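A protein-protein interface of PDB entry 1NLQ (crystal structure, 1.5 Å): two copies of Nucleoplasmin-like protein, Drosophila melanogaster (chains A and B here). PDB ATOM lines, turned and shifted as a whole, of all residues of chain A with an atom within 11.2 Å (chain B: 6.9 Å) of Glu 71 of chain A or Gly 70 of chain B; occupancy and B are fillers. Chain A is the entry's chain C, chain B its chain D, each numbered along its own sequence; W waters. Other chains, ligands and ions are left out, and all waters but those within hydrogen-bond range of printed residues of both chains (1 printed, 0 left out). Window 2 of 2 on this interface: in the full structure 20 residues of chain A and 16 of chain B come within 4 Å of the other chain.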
ATOM      1  N   ILE A  37      26.951 -26.789 -22.299  1.00  0.00           N
ATOM      2  CA  ILE A  37      26.638 -25.807 -23.324  1.00  0.00           C
ATOM      3  C   ILE A  37      25.179 -25.496 -22.990  1.00  0.00           C
ATOM      4  O   ILE A  37      24.313 -26.370 -23.038  1.00  0.00           O
ATOM      5  CB  ILE A  37      26.827 -26.375 -24.741  1.00  0.00           C
ATOM      6  CG1 ILE A  37      28.303 -26.749 -24.936  1.00  0.00           C
ATOM      7  CG2 ILE A  37      26.446 -25.319 -25.777  1.00  0.00           C
ATOM      8  CD1 ILE A  37      28.617 -27.430 -26.261  1.00  0.00           C
ATOM      9  N   LEU A  38      24.930 -24.238 -22.637  1.00  0.00           N
ATOM     10  CA  LEU A  38      23.628 -23.771 -22.177  1.00  0.00           C
ATOM     11  C   LEU A  38      22.983 -22.682 -23.035  1.00  0.00           C
ATOM     12  O   LEU A  38      23.635 -21.725 -23.426  1.00  0.00           O
ATOM     13  CB  LEU A  38      23.807 -23.264 -20.736  1.00  0.00           C
ATOM     14  CG  LEU A  38      22.645 -22.637 -19.967  1.00  0.00           C
ATOM     15  CD1 LEU A  38      21.631 -23.705 -19.597  1.00  0.00           C
ATOM     16  CD2 LEU A  38      23.191 -21.966 -18.697  1.00  0.00           C
ATOM     17  N   LEU A  39      21.685 -22.828 -23.289  1.00  0.00           N
ATOM     18  CA  LEU A  39      20.941 -21.866 -24.097  1.00  0.00           C
ATOM     19  C   LEU A  39      20.441 -20.702 -23.235  1.00  0.00           C
ATOM     20  O   LEU A  39      19.801 -20.911 -22.200  1.00  0.00           O
ATOM     21  CB  LEU A  39      19.751 -22.565 -24.765  1.00  0.00           C
ATOM     22  CG  LEU A  39      18.949 -21.737 -25.773  1.00  0.00           C
ATOM     23  CD1 LEU A  39      19.834 -21.377 -26.965  1.00  0.00           C
ATOM     24  CD2 LEU A  39      17.732 -22.536 -26.237  1.00  0.00           C
ATOM     25  N   GLY A  40      20.723 -19.478 -23.679  1.00  0.00           N
ATOM     26  CA  GLY A  40      20.300 -18.304 -22.936  1.00  0.00           C
ATOM     27  C   GLY A  40      18.794 -18.129 -22.872  1.00  0.00           C
ATOM     28  O   GLY A  40      18.074 -18.534 -23.785  1.00  0.00           O
ATOM     29  N   ALA A  43      16.887 -16.685 -25.852  1.00  0.00           N
ATOM     30  CA  ALA A  43      16.853 -17.413 -27.111  1.00  0.00           C
ATOM     31  C   ALA A  43      15.419 -17.550 -27.584  1.00  0.00           C
ATOM     32  O   ALA A  43      14.539 -17.906 -26.812  1.00  0.00           O
ATOM     33  CB  ALA A  43      17.482 -18.785 -26.945  1.00  0.00           C
ATOM     34  N   LYS A  44      15.195 -17.267 -28.860  1.00  0.00           N
ATOM     35  CA  LYS A  44      13.862 -17.359 -29.446  1.00  0.00           C
ATOM     36  C   LYS A  44      13.249 -18.750 -29.252  1.00  0.00           C
ATOM     37  O   LYS A  44      13.905 -19.765 -29.484  1.00  0.00           O
ATOM     38  CB  LYS A  44      13.928 -17.040 -30.947  1.00  0.00           C
ATOM     39  CG  LYS A  44      14.225 -15.580 -31.278  1.00  0.00           C
ATOM     40  CD  LYS A  44      13.097 -14.690 -30.771  1.00  0.00           C
ATOM     41  CE  LYS A  44      13.260 -13.241 -31.194  1.00  0.00           C
ATOM     42  NZ  LYS A  44      12.116 -12.456 -30.639  1.00  0.00           N
ATOM     43  N   GLU A  45      11.986 -18.792 -28.833  1.00  0.00           N
ATOM     44  CA  GLU A  45      11.310 -20.070 -28.632  1.00  0.00           C
ATOM     45  C   GLU A  45      11.294 -20.859 -29.942  1.00  0.00           C
ATOM     46  O   GLU A  45      11.139 -20.281 -31.021  1.00  0.00           O
ATOM     47  CB  GLU A  45       9.868 -19.848 -28.156  1.00  0.00           C
ATOM     48  CG  GLU A  45       9.136 -21.127 -27.713  1.00  0.00           C
ATOM     49  CD  GLU A  45       9.542 -21.607 -26.322  1.00  0.00           C
ATOM     50  OE1 GLU A  45      10.411 -20.965 -25.702  1.00  0.00           O
ATOM     51  OE2 GLU A  45       8.985 -22.625 -25.850  1.00  0.00           O
ATOM     52  N   ASN A  46      11.473 -22.174 -29.843  1.00  0.00           N
ATOM     53  CA  ASN A  46      11.461 -23.065 -31.007  1.00  0.00           C
ATOM     54  C   ASN A  46      12.604 -22.888 -32.010  1.00  0.00           C
ATOM     55  O   ASN A  46      12.612 -23.531 -33.063  1.00  0.00           O
ATOM     56  CB  ASN A  46      10.124 -22.944 -31.755  1.00  0.00           C
ATOM     57  CG  ASN A  46       8.925 -23.202 -30.856  1.00  0.00           C
ATOM     58  OD1 ASN A  46       8.850 -24.230 -30.187  1.00  0.00           O
ATOM     59  ND2 ASN A  46       7.979 -22.264 -30.833  1.00  0.00           N
ATOM     60  N   GLU A  47      13.561 -22.026 -31.698  1.00  0.00           N
ATOM     61  CA  GLU A  47      14.685 -21.794 -32.600  1.00  0.00           C
ATOM     62  C   GLU A  47      15.861 -22.717 -32.316  1.00  0.00           C
ATOM     63  O   GLU A  47      16.410 -22.721 -31.218  1.00  0.00           O
ATOM     64  CB  GLU A  47      15.163 -20.350 -32.494  1.00  0.00           C
ATOM     65  CG  GLU A  47      16.349 -20.014 -33.378  1.00  0.00           C
ATOM     66  CD  GLU A  47      16.857 -18.614 -33.124  1.00  0.00           C
ATOM     67  OE1 GLU A  47      17.921 -18.452 -32.480  1.00  0.00           O
ATOM     68  OE2 GLU A  47      16.175 -17.672 -33.556  1.00  0.00           O
ATOM     69  N   PHE A  48      16.253 -23.488 -33.319  1.00  0.00           N
ATOM     70  CA  PHE A  48      17.386 -24.385 -33.158  1.00  0.00           C
ATOM     71  C   PHE A  48      18.684 -23.608 -33.119  1.00  0.00           C
ATOM     72  O   PHE A  48      18.952 -22.760 -33.974  1.00  0.00           O
ATOM     73  CB  PHE A  48      17.454 -25.394 -34.302  1.00  0.00           C
ATOM     74  CG  PHE A  48      16.586 -26.598 -34.104  1.00  0.00           C
ATOM     75  CD1 PHE A  48      15.522 -26.854 -34.966  1.00  0.00           C
ATOM     76  CD2 PHE A  48      16.841 -27.494 -33.067  1.00  0.00           C
ATOM     77  CE1 PHE A  48      14.725 -27.991 -34.796  1.00  0.00           C
ATOM     78  CE2 PHE A  48      16.050 -28.631 -32.891  1.00  0.00           C
ATOM     79  CZ  PHE A  48      14.986 -28.880 -33.763  1.00  0.00           C
ATOM     80  N   ASN A  49      19.484 -23.897 -32.102  1.00  0.00           N
ATOM     81  CA  ASN A  49      20.784 -23.275 -31.928  1.00  0.00           C
ATOM     82  C   ASN A  49      21.784 -24.409 -31.911  1.00  0.00           C
ATOM     83  O   ASN A  49      21.741 -25.274 -31.037  1.00  0.00           O
ATOM     84  CB  ASN A  49      20.832 -22.489 -30.623  1.00  0.00           C
ATOM     85  CG  ASN A  49      20.244 -21.107 -30.774  1.00  0.00           C
ATOM     86  OD1 ASN A  49      20.969 -20.116 -30.822  1.00  0.00           O
ATOM     87  ND2 ASN A  49      18.920 -21.035 -30.877  1.00  0.00           N
ATOM     88  N   VAL A  50      22.678 -24.400 -32.891  1.00  0.00           N
ATOM     89  CA  VAL A  50      23.664 -25.457 -33.037  1.00  0.00           C
ATOM     90  C   VAL A  50      25.088 -24.939 -32.910  1.00  0.00           C
ATOM     91  O   VAL A  50      25.478 -23.991 -33.589  1.00  0.00           O
ATOM     92  CB  VAL A  50      23.505 -26.134 -34.421  1.00  0.00           C
ATOM     93  CG1 VAL A  50      24.535 -27.242 -34.601  1.00  0.00           C
ATOM     94  CG2 VAL A  50      22.094 -26.695 -34.555  1.00  0.00           C
ATOM     95  N   ALA A  65      26.473 -29.510 -29.864  1.00  0.00           N
ATOM     96  CA  ALA A  65      25.307 -29.076 -29.117  1.00  0.00           C
ATOM     97  C   ALA A  65      24.201 -28.677 -30.071  1.00  0.00           C
ATOM     98  O   ALA A  65      24.443 -27.987 -31.058  1.00  0.00           O
ATOM     99  CB  ALA A  65      25.647 -27.895 -28.214  1.00  0.00           C
ATOM    100  N   VAL A  66      23.002 -29.159 -29.780  1.00  0.00           N
ATOM    101  CA  VAL A  66      21.804 -28.816 -30.544  1.00  0.00           C
ATOM    102  C   VAL A  66      20.822 -28.444 -29.445  1.00  0.00           C
ATOM    103  O   VAL A  66      20.403 -29.295 -28.650  1.00  0.00           O
ATOM    104  CB  VAL A  66      21.260 -30.000 -31.359  1.00  0.00           C
ATOM    105  CG1 VAL A  66      19.943 -29.602 -32.024  1.00  0.00           C
ATOM    106  CG2 VAL A  66      22.267 -30.391 -32.432  1.00  0.00           C
ATOM    107  N   LEU A  67      20.486 -27.160 -29.383  1.00  0.00           N
ATOM    108  CA  LEU A  67      19.591 -26.647 -28.356  1.00  0.00           C
ATOM    109  C   LEU A  67      18.379 -25.975 -28.981  1.00  0.00           C
ATOM    110  O   LEU A  67      18.422 -25.542 -30.133  1.00  0.00           O
ATOM    111  CB  LEU A  67      20.341 -25.636 -27.487  1.00  0.00           C
ATOM    112  CG  LEU A  67      21.660 -26.105 -26.868  1.00  0.00           C
ATOM    113  CD1 LEU A  67      22.382 -24.929 -26.228  1.00  0.00           C
ATOM    114  CD2 LEU A  67      21.377 -27.183 -25.819  1.00  0.00           C
ATOM    115  N   LYS A  68      17.300 -25.889 -28.210  1.00  0.00           N
ATOM    116  CA  LYS A  68      16.078 -25.254 -28.678  1.00  0.00           C
ATOM    117  C   LYS A  68      15.162 -24.938 -27.512  1.00  0.00           C
ATOM    118  O   LYS A  68      14.747 -25.836 -26.778  1.00  0.00           O
ATOM    119  CB  LYS A  68      15.343 -26.150 -29.682  1.00  0.00           C
ATOM    120  CG  LYS A  68      14.117 -25.460 -30.290  1.00  0.00           C
ATOM    121  CD  LYS A  68      13.515 -26.225 -31.478  1.00  0.00           C
ATOM    122  CE  LYS A  68      12.861 -27.519 -31.042  1.00  0.00           C
ATOM    123  NZ  LYS A  68      11.893 -27.987 -32.096  1.00  0.00           N
ATOM    124  N   ALA A  69      14.857 -23.657 -27.342  1.00  0.00           N
ATOM    125  CA  ALA A  69      13.979 -23.221 -26.264  1.00  0.00           C
ATOM    126  C   ALA A  69      12.657 -23.951 -26.418  1.00  0.00           C
ATOM    127  O   ALA A  69      12.055 -23.944 -27.503  1.00  0.00           O
ATOM    128  CB  ALA A  69      13.766 -21.719 -26.341  1.00  0.00           C
ATOM    129  N   GLY A  70      12.210 -24.570 -25.332  1.00  0.00           N
ATOM    130  CA  GLY A  70      10.970 -25.319 -25.352  1.00  0.00           C
ATOM    131  C   GLY A  70      11.216 -26.812 -25.434  1.00  0.00           C
ATOM    132  O   GLY A  70      10.298 -27.599 -25.206  1.00  0.00           O
ATOM    133  N   GLU A  71      12.446 -27.212 -25.757  1.00  0.00           N
ATOM    134  CA  GLU A  71      12.779 -28.635 -25.869  1.00  0.00           C
ATOM    135  C   GLU A  71      14.049 -29.054 -25.139  1.00  0.00           C
ATOM    136  O   GLU A  71      14.023 -29.953 -24.297  1.00  0.00           O
ATOM    137  CB  GLU A  71      12.932 -29.050 -27.337  1.00  0.00           C
ATOM    138  CG  GLU A  71      13.263 -30.531 -27.478  1.00  0.00           C
ATOM    139  CD  GLU A  71      14.064 -30.861 -28.726  1.00  0.00           C
ATOM    140  OE1 GLU A  71      13.481 -31.347 -29.713  1.00  0.00           O
ATOM    141  OE2 GLU A  71      15.286 -30.634 -28.709  1.00  0.00           O
ATOM    142  N   THR A  72      15.157 -28.409 -25.481  1.00  0.00           N
ATOM    143  CA  THR A  72      16.444 -28.736 -24.884  1.00  0.00           C
ATOM    144  C   THR A  72      17.151 -27.446 -24.487  1.00  0.00           C
ATOM    145  O   THR A  72      17.558 -26.663 -25.334  1.00  0.00           O
ATOM    146  CB  THR A  72      17.300 -29.522 -25.893  1.00  0.00           C
ATOM    147  OG1 THR A  72      16.552 -30.645 -26.372  1.00  0.00           O
ATOM    148  CG2 THR A  72      18.579 -30.016 -25.248  1.00  0.00           C
ATOM    149  N   ARG A  73      17.283 -27.241 -23.181  1.00  0.00           N
ATOM    150  CA  ARG A  73      17.900 -26.044 -22.630  1.00  0.00           C
ATOM    151  C   ARG A  73      19.409 -26.154 -22.484  1.00  0.00           C
ATOM    152  O   ARG A  73      20.117 -25.152 -22.525  1.00  0.00           O
ATOM    153  CB  ARG A  73      17.246 -25.738 -21.268  1.00  0.00           C
ATOM    154  CG  ARG A  73      17.799 -24.532 -20.503  1.00  0.00           C
ATOM    155  CD  ARG A  73      17.664 -23.229 -21.274  1.00  0.00           C
ATOM    156  NE  ARG A  73      16.303 -22.984 -21.745  1.00  0.00           N
ATOM    157  CZ  ARG A  73      15.962 -21.934 -22.483  1.00  0.00           C
ATOM    158  NH1 ARG A  73      16.875 -21.035 -22.819  1.00  0.00           N
ATOM    159  NH2 ARG A  73      14.717 -21.799 -22.915  1.00  0.00           N
ATOM    160  N   ALA A  74      19.901 -27.374 -22.313  1.00  0.00           N
ATOM    161  CA  ALA A  74      21.334 -27.565 -22.144  1.00  0.00           C
ATOM    162  C   ALA A  74      21.773 -28.988 -22.458  1.00  0.00           C
ATOM    163  O   ALA A  74      20.967 -29.914 -22.452  1.00  0.00           O
ATOM    164  CB  ALA A  74      21.733 -27.219 -20.701  1.00  0.00           C
ATOM    165  N   VAL A  75      23.060 -29.132 -22.750  1.00  0.00           N
ATOM    166  CA  VAL A  75      23.669 -30.430 -22.992  1.00  0.00           C
ATOM    167  C   VAL A  75      24.942 -30.447 -22.156  1.00  0.00           C
ATOM    168  O   VAL A  75      25.487 -29.395 -21.806  1.00  0.00           O
ATOM    169  CB  VAL A  75      24.018 -30.700 -24.494  1.00  0.00           C
ATOM    170  CG1 VAL A  75      22.742 -30.876 -25.299  1.00  0.00           C
ATOM    171  CG2 VAL A  75      24.895 -29.587 -25.060  1.00  0.00           C
ATOM    172  N   LEU B  39      21.242 -35.783 -31.210  1.00  0.00           N
ATOM    173  CA  LEU B  39      20.370 -35.762 -32.377  1.00  0.00           C
ATOM    174  C   LEU B  39      20.458 -34.419 -33.089  1.00  0.00           C
ATOM    175  O   LEU B  39      20.321 -33.367 -32.466  1.00  0.00           O
ATOM    176  CB  LEU B  39      18.928 -36.026 -31.947  1.00  0.00           C
ATOM    177  CG  LEU B  39      17.905 -36.166 -33.070  1.00  0.00           C
ATOM    178  CD1 LEU B  39      18.225 -37.413 -33.884  1.00  0.00           C
ATOM    179  CD2 LEU B  39      16.508 -36.271 -32.481  1.00  0.00           C
ATOM    180  N   LYS B  44      13.872 -35.469 -38.211  1.00  0.00           N
ATOM    181  CA  LYS B  44      12.413 -35.396 -38.305  1.00  0.00           C
ATOM    182  C   LYS B  44      11.702 -35.434 -36.950  1.00  0.00           C
ATOM    183  O   LYS B  44      11.914 -36.341 -36.138  1.00  0.00           O
ATOM    184  CB  LYS B  44      11.877 -36.524 -39.196  1.00  0.00           C
ATOM    185  CG  LYS B  44      10.392 -36.373 -39.519  1.00  0.00           C
ATOM    186  CD  LYS B  44       9.984 -37.157 -40.762  1.00  0.00           C
ATOM    187  CE  LYS B  44       9.349 -38.474 -40.389  1.00  0.00           C
ATOM    188  NZ  LYS B  44      10.266 -39.295 -39.576  1.00  0.00           N
ATOM    189  N   GLU B  45      10.839 -34.451 -36.716  1.00  0.00           N
ATOM    190  CA  GLU B  45      10.131 -34.389 -35.447  1.00  0.00           C
ATOM    191  C   GLU B  45       9.381 -35.687 -35.233  1.00  0.00           C
ATOM    192  O   GLU B  45       8.746 -36.199 -36.158  1.00  0.00           O
ATOM    193  CB  GLU B  45       9.147 -33.212 -35.427  1.00  0.00           C
ATOM    194  CG  GLU B  45       8.461 -32.971 -34.087  1.00  0.00           C
ATOM    195  CD  GLU B  45       9.376 -32.296 -33.066  1.00  0.00           C
ATOM    196  OE1 GLU B  45       8.938 -32.115 -31.907  1.00  0.00           O
ATOM    197  OE2 GLU B  45      10.520 -31.933 -33.423  1.00  0.00           O
ATOM    198  N   ASN B  46       9.491 -36.227 -34.023  1.00  0.00           N
ATOM    199  CA  ASN B  46       8.803 -37.458 -33.647  1.00  0.00           C
ATOM    200  C   ASN B  46       9.365 -38.738 -34.252  1.00  0.00           C
ATOM    201  O   ASN B  46       8.767 -39.797 -34.118  1.00  0.00           O
ATOM    202  CB  ASN B  46       7.329 -37.347 -34.025  1.00  0.00           C
ATOM    203  CG  ASN B  46       6.418 -37.350 -32.830  1.00  0.00           C
ATOM    204  OD1 ASN B  46       5.224 -37.058 -32.952  1.00  0.00           O
ATOM    205  ND2 ASN B  46       6.958 -37.690 -31.666  1.00  0.00           N
ATOM    206  N   LYS B  68      14.784 -38.913 -30.119  1.00  0.00           N
ATOM    207  CA  LYS B  68      13.578 -38.500 -30.843  1.00  0.00           C
ATOM    208  C   LYS B  68      13.275 -37.026 -30.643  1.00  0.00           C
ATOM    209  O   LYS B  68      13.033 -36.581 -29.520  1.00  0.00           O
ATOM    210  CB  LYS B  68      12.369 -39.330 -30.403  1.00  0.00           C
ATOM    211  CG  LYS B  68      11.128 -39.043 -31.243  1.00  0.00           C
ATOM    212  CD  LYS B  68      10.014 -40.055 -31.034  1.00  0.00           C
ATOM    213  CE  LYS B  68       9.327 -39.872 -29.702  1.00  0.00           C
ATOM    214  NZ  LYS B  68       8.076 -40.686 -29.648  1.00  0.00           N
ATOM    215  N   ALA B  69      13.284 -36.278 -31.742  1.00  0.00           N
ATOM    216  CA  ALA B  69      13.008 -34.848 -31.708  1.00  0.00           C
ATOM    217  C   ALA B  69      11.675 -34.653 -31.001  1.00  0.00           C
ATOM    218  O   ALA B  69      10.677 -35.277 -31.364  1.00  0.00           O
ATOM    219  CB  ALA B  69      12.947 -34.295 -33.130  1.00  0.00           C
ATOM    220  N   GLY B  70      11.671 -33.805 -29.980  1.00  0.00           N
ATOM    221  CA  GLY B  70      10.457 -33.561 -29.222  1.00  0.00           C
ATOM    222  C   GLY B  70      10.408 -34.330 -27.914  1.00  0.00           C
ATOM    223  O   GLY B  70       9.551 -34.063 -27.071  1.00  0.00           O
ATOM    224  N   GLU B  71      11.314 -35.290 -27.731  1.00  0.00           N
ATOM    225  CA  GLU B  71      11.345 -36.068 -26.492  1.00  0.00           C
ATOM    226  C   GLU B  71      12.751 -36.178 -25.920  1.00  0.00           C
ATOM    227  O   GLU B  71      13.007 -35.731 -24.804  1.00  0.00           O
ATOM    228  CB  GLU B  71      10.793 -37.479 -26.703  1.00  0.00           C
ATOM    229  CG  GLU B  71      10.794 -38.307 -25.423  1.00  0.00           C
ATOM    230  CD  GLU B  71      10.937 -39.796 -25.680  1.00  0.00           C
ATOM    231  OE1 GLU B  71       9.917 -40.513 -25.624  1.00  0.00           O
ATOM    232  OE2 GLU B  71      12.070 -40.244 -25.944  1.00  0.00           O
ATOM    233  N   THR B  72      13.663 -36.760 -26.695  1.00  0.00           N
ATOM    234  CA  THR B  72      15.036 -36.940 -26.240  1.00  0.00           C
ATOM    235  C   THR B  72      16.036 -36.432 -27.285  1.00  0.00           C
ATOM    236  O   THR B  72      16.209 -37.038 -28.343  1.00  0.00           O
ATOM    237  CB  THR B  72      15.282 -38.430 -25.933  1.00  0.00           C
ATOM    238  OG1 THR B  72      14.263 -38.898 -25.035  1.00  0.00           O
ATOM    239  CG2 THR B  72      16.631 -38.628 -25.273  1.00  0.00           C
ATOM    240  N   ARG B  73      16.697 -35.322 -26.977  1.00  0.00           N
ATOM    241  CA  ARG B  73      17.657 -34.704 -27.888  1.00  0.00           C
ATOM    242  C   ARG B  73      19.051 -35.315 -27.784  1.00  0.00           C
ATOM    243  O   ARG B  73      19.819 -35.295 -28.750  1.00  0.00           O
ATOM    244  CB  ARG B  73      17.718 -33.195 -27.613  1.00  0.00           C
ATOM    245  CG  ARG B  73      18.732 -32.403 -28.446  1.00  0.00           C
ATOM    246  CD  ARG B  73      18.485 -32.502 -29.948  1.00  0.00           C
ATOM    247  NE  ARG B  73      17.109 -32.172 -30.317  1.00  0.00           N
ATOM    248  CZ  ARG B  73      16.643 -32.247 -31.558  1.00  0.00           C
ATOM    249  NH1 ARG B  73      17.449 -32.625 -32.543  1.00  0.00           N
ATOM    250  NH2 ARG B  73      15.369 -31.977 -31.812  1.00  0.00           N
HETATM  251  O   HOH W   1      12.354 -30.462 -32.237  1.00  0.00           O
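OE1 of Glu 71 of chain A is in hydrogen-bond range of N of Gly 70 of chain B, at 3.1 Å.
The side-chain carboxylate (OE2) of Glu 71 of chain A is in salt-bridge range of the guanidinium group (NE) of Arg 73 of chain B (2.9 Å).
The side-chain carboxylate (OE2) of Glu 71 of chain A sits at hydrogen-bond distance from the side-chain hydroxyl (OG1) of Thr 72 of chain A, 2.7 Å away.
The backbone NH (N) of Leu 39 of chain B is in hydrogen-bond range of the backbone carbonyl oxygen (O) of Arg 73 of chain B (2.9 Å).
The backbone NH of Asn 46 of chain B lies within hydrogen-bond range of the backbone carbonyl oxygen of Ala 69 of chain B, 3.1 Å away.
Among the printed residues, merely in contact across the chains: Phe 48 of chain A with Arg 73 of chain B, Val 66 of chain A with Leu 39 of chain B, Val 66 of chain A with Arg 73 of chain B, Glu 71 of chain A with Ala 69 of chain B and Thr 72 of chain A with Arg 73 of chain B.
Of the printed residues of chain B, Glu 71 of chain A touches Ala 69, Gly 70 and Arg 73.
Gly 70 of chain B touches just one residue of chain A: Glu 71.
No residue of chain A comes within 4 Å of Lys 68 of chain B.
Of the printed residues of chain A, Arg 73 of chain B touches Phe 48 (3.6 Å), Val 66 (3.5 Å), Glu 71 (2.9 Å) and Thr 72 (3.1 Å).
Printed residues of chain A within 4 Å of Leu 39 of chain B: Val 66.
Of the printed residues of chain B, Phe 48 of chain A touches Arg 73 (3.6 Å).
Printed residues of chain A within 4 Å of Ala 69 of chain B: Glu 71 (3.98 Å).
The nearest residue of chain A that does not touch Gly 70 of chain B is Lys 68 of chain A (6.2 Å).
Of the 10 printed residues of chain B, 4 touch a printed residue of chain A.
Among the printed residues, 7 pairs touch across the chains.
Among the printed residues, Asp or Glu carboxylates within 4 Å of a Lys or Arg side-chain nitrogen of the other chain: Glu 71 of chain A with Arg 73 of chain B.
Glu 71 of chain A touches Ala 69 of chain B, but with the chains exchanged Ala 69 of chain A does not touch Glu 71 of chain B (11.4 Å).
Glu 71 of chain A touches Gly 70 of chain B, but with the chains exchanged Gly 70 of chain A does not touch Glu 71 of chain B (8.2 Å).
Glu 71 of chain A touches Arg 73 of chain B, but with the chains exchanged Arg 73 of chain A does not touch Glu 71 of chain B (9.6 Å).
Thr 72 of chain A touches Arg 73 of chain B, but with the chains exchanged Arg 73 of chain A does not touch Thr 72 of chain B (10.1 Å).
10 positions are printed for both chains.
Of the 7 pairs that touch across the chains among the printed residues, none has its exchanged pair printed and touching as well.
Water W1 lies within hydrogen-bond range of the side-chain amino group of Lys 68 of chain A (2.5 Å), the side-chain carboxylate of Glu 45 of chain B (2.6 Å), the side-chain carboxylate of Glu 71 of chain A (2.9 Å) and the guanidinium group of Arg 73 of chain B (3.4 Å).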
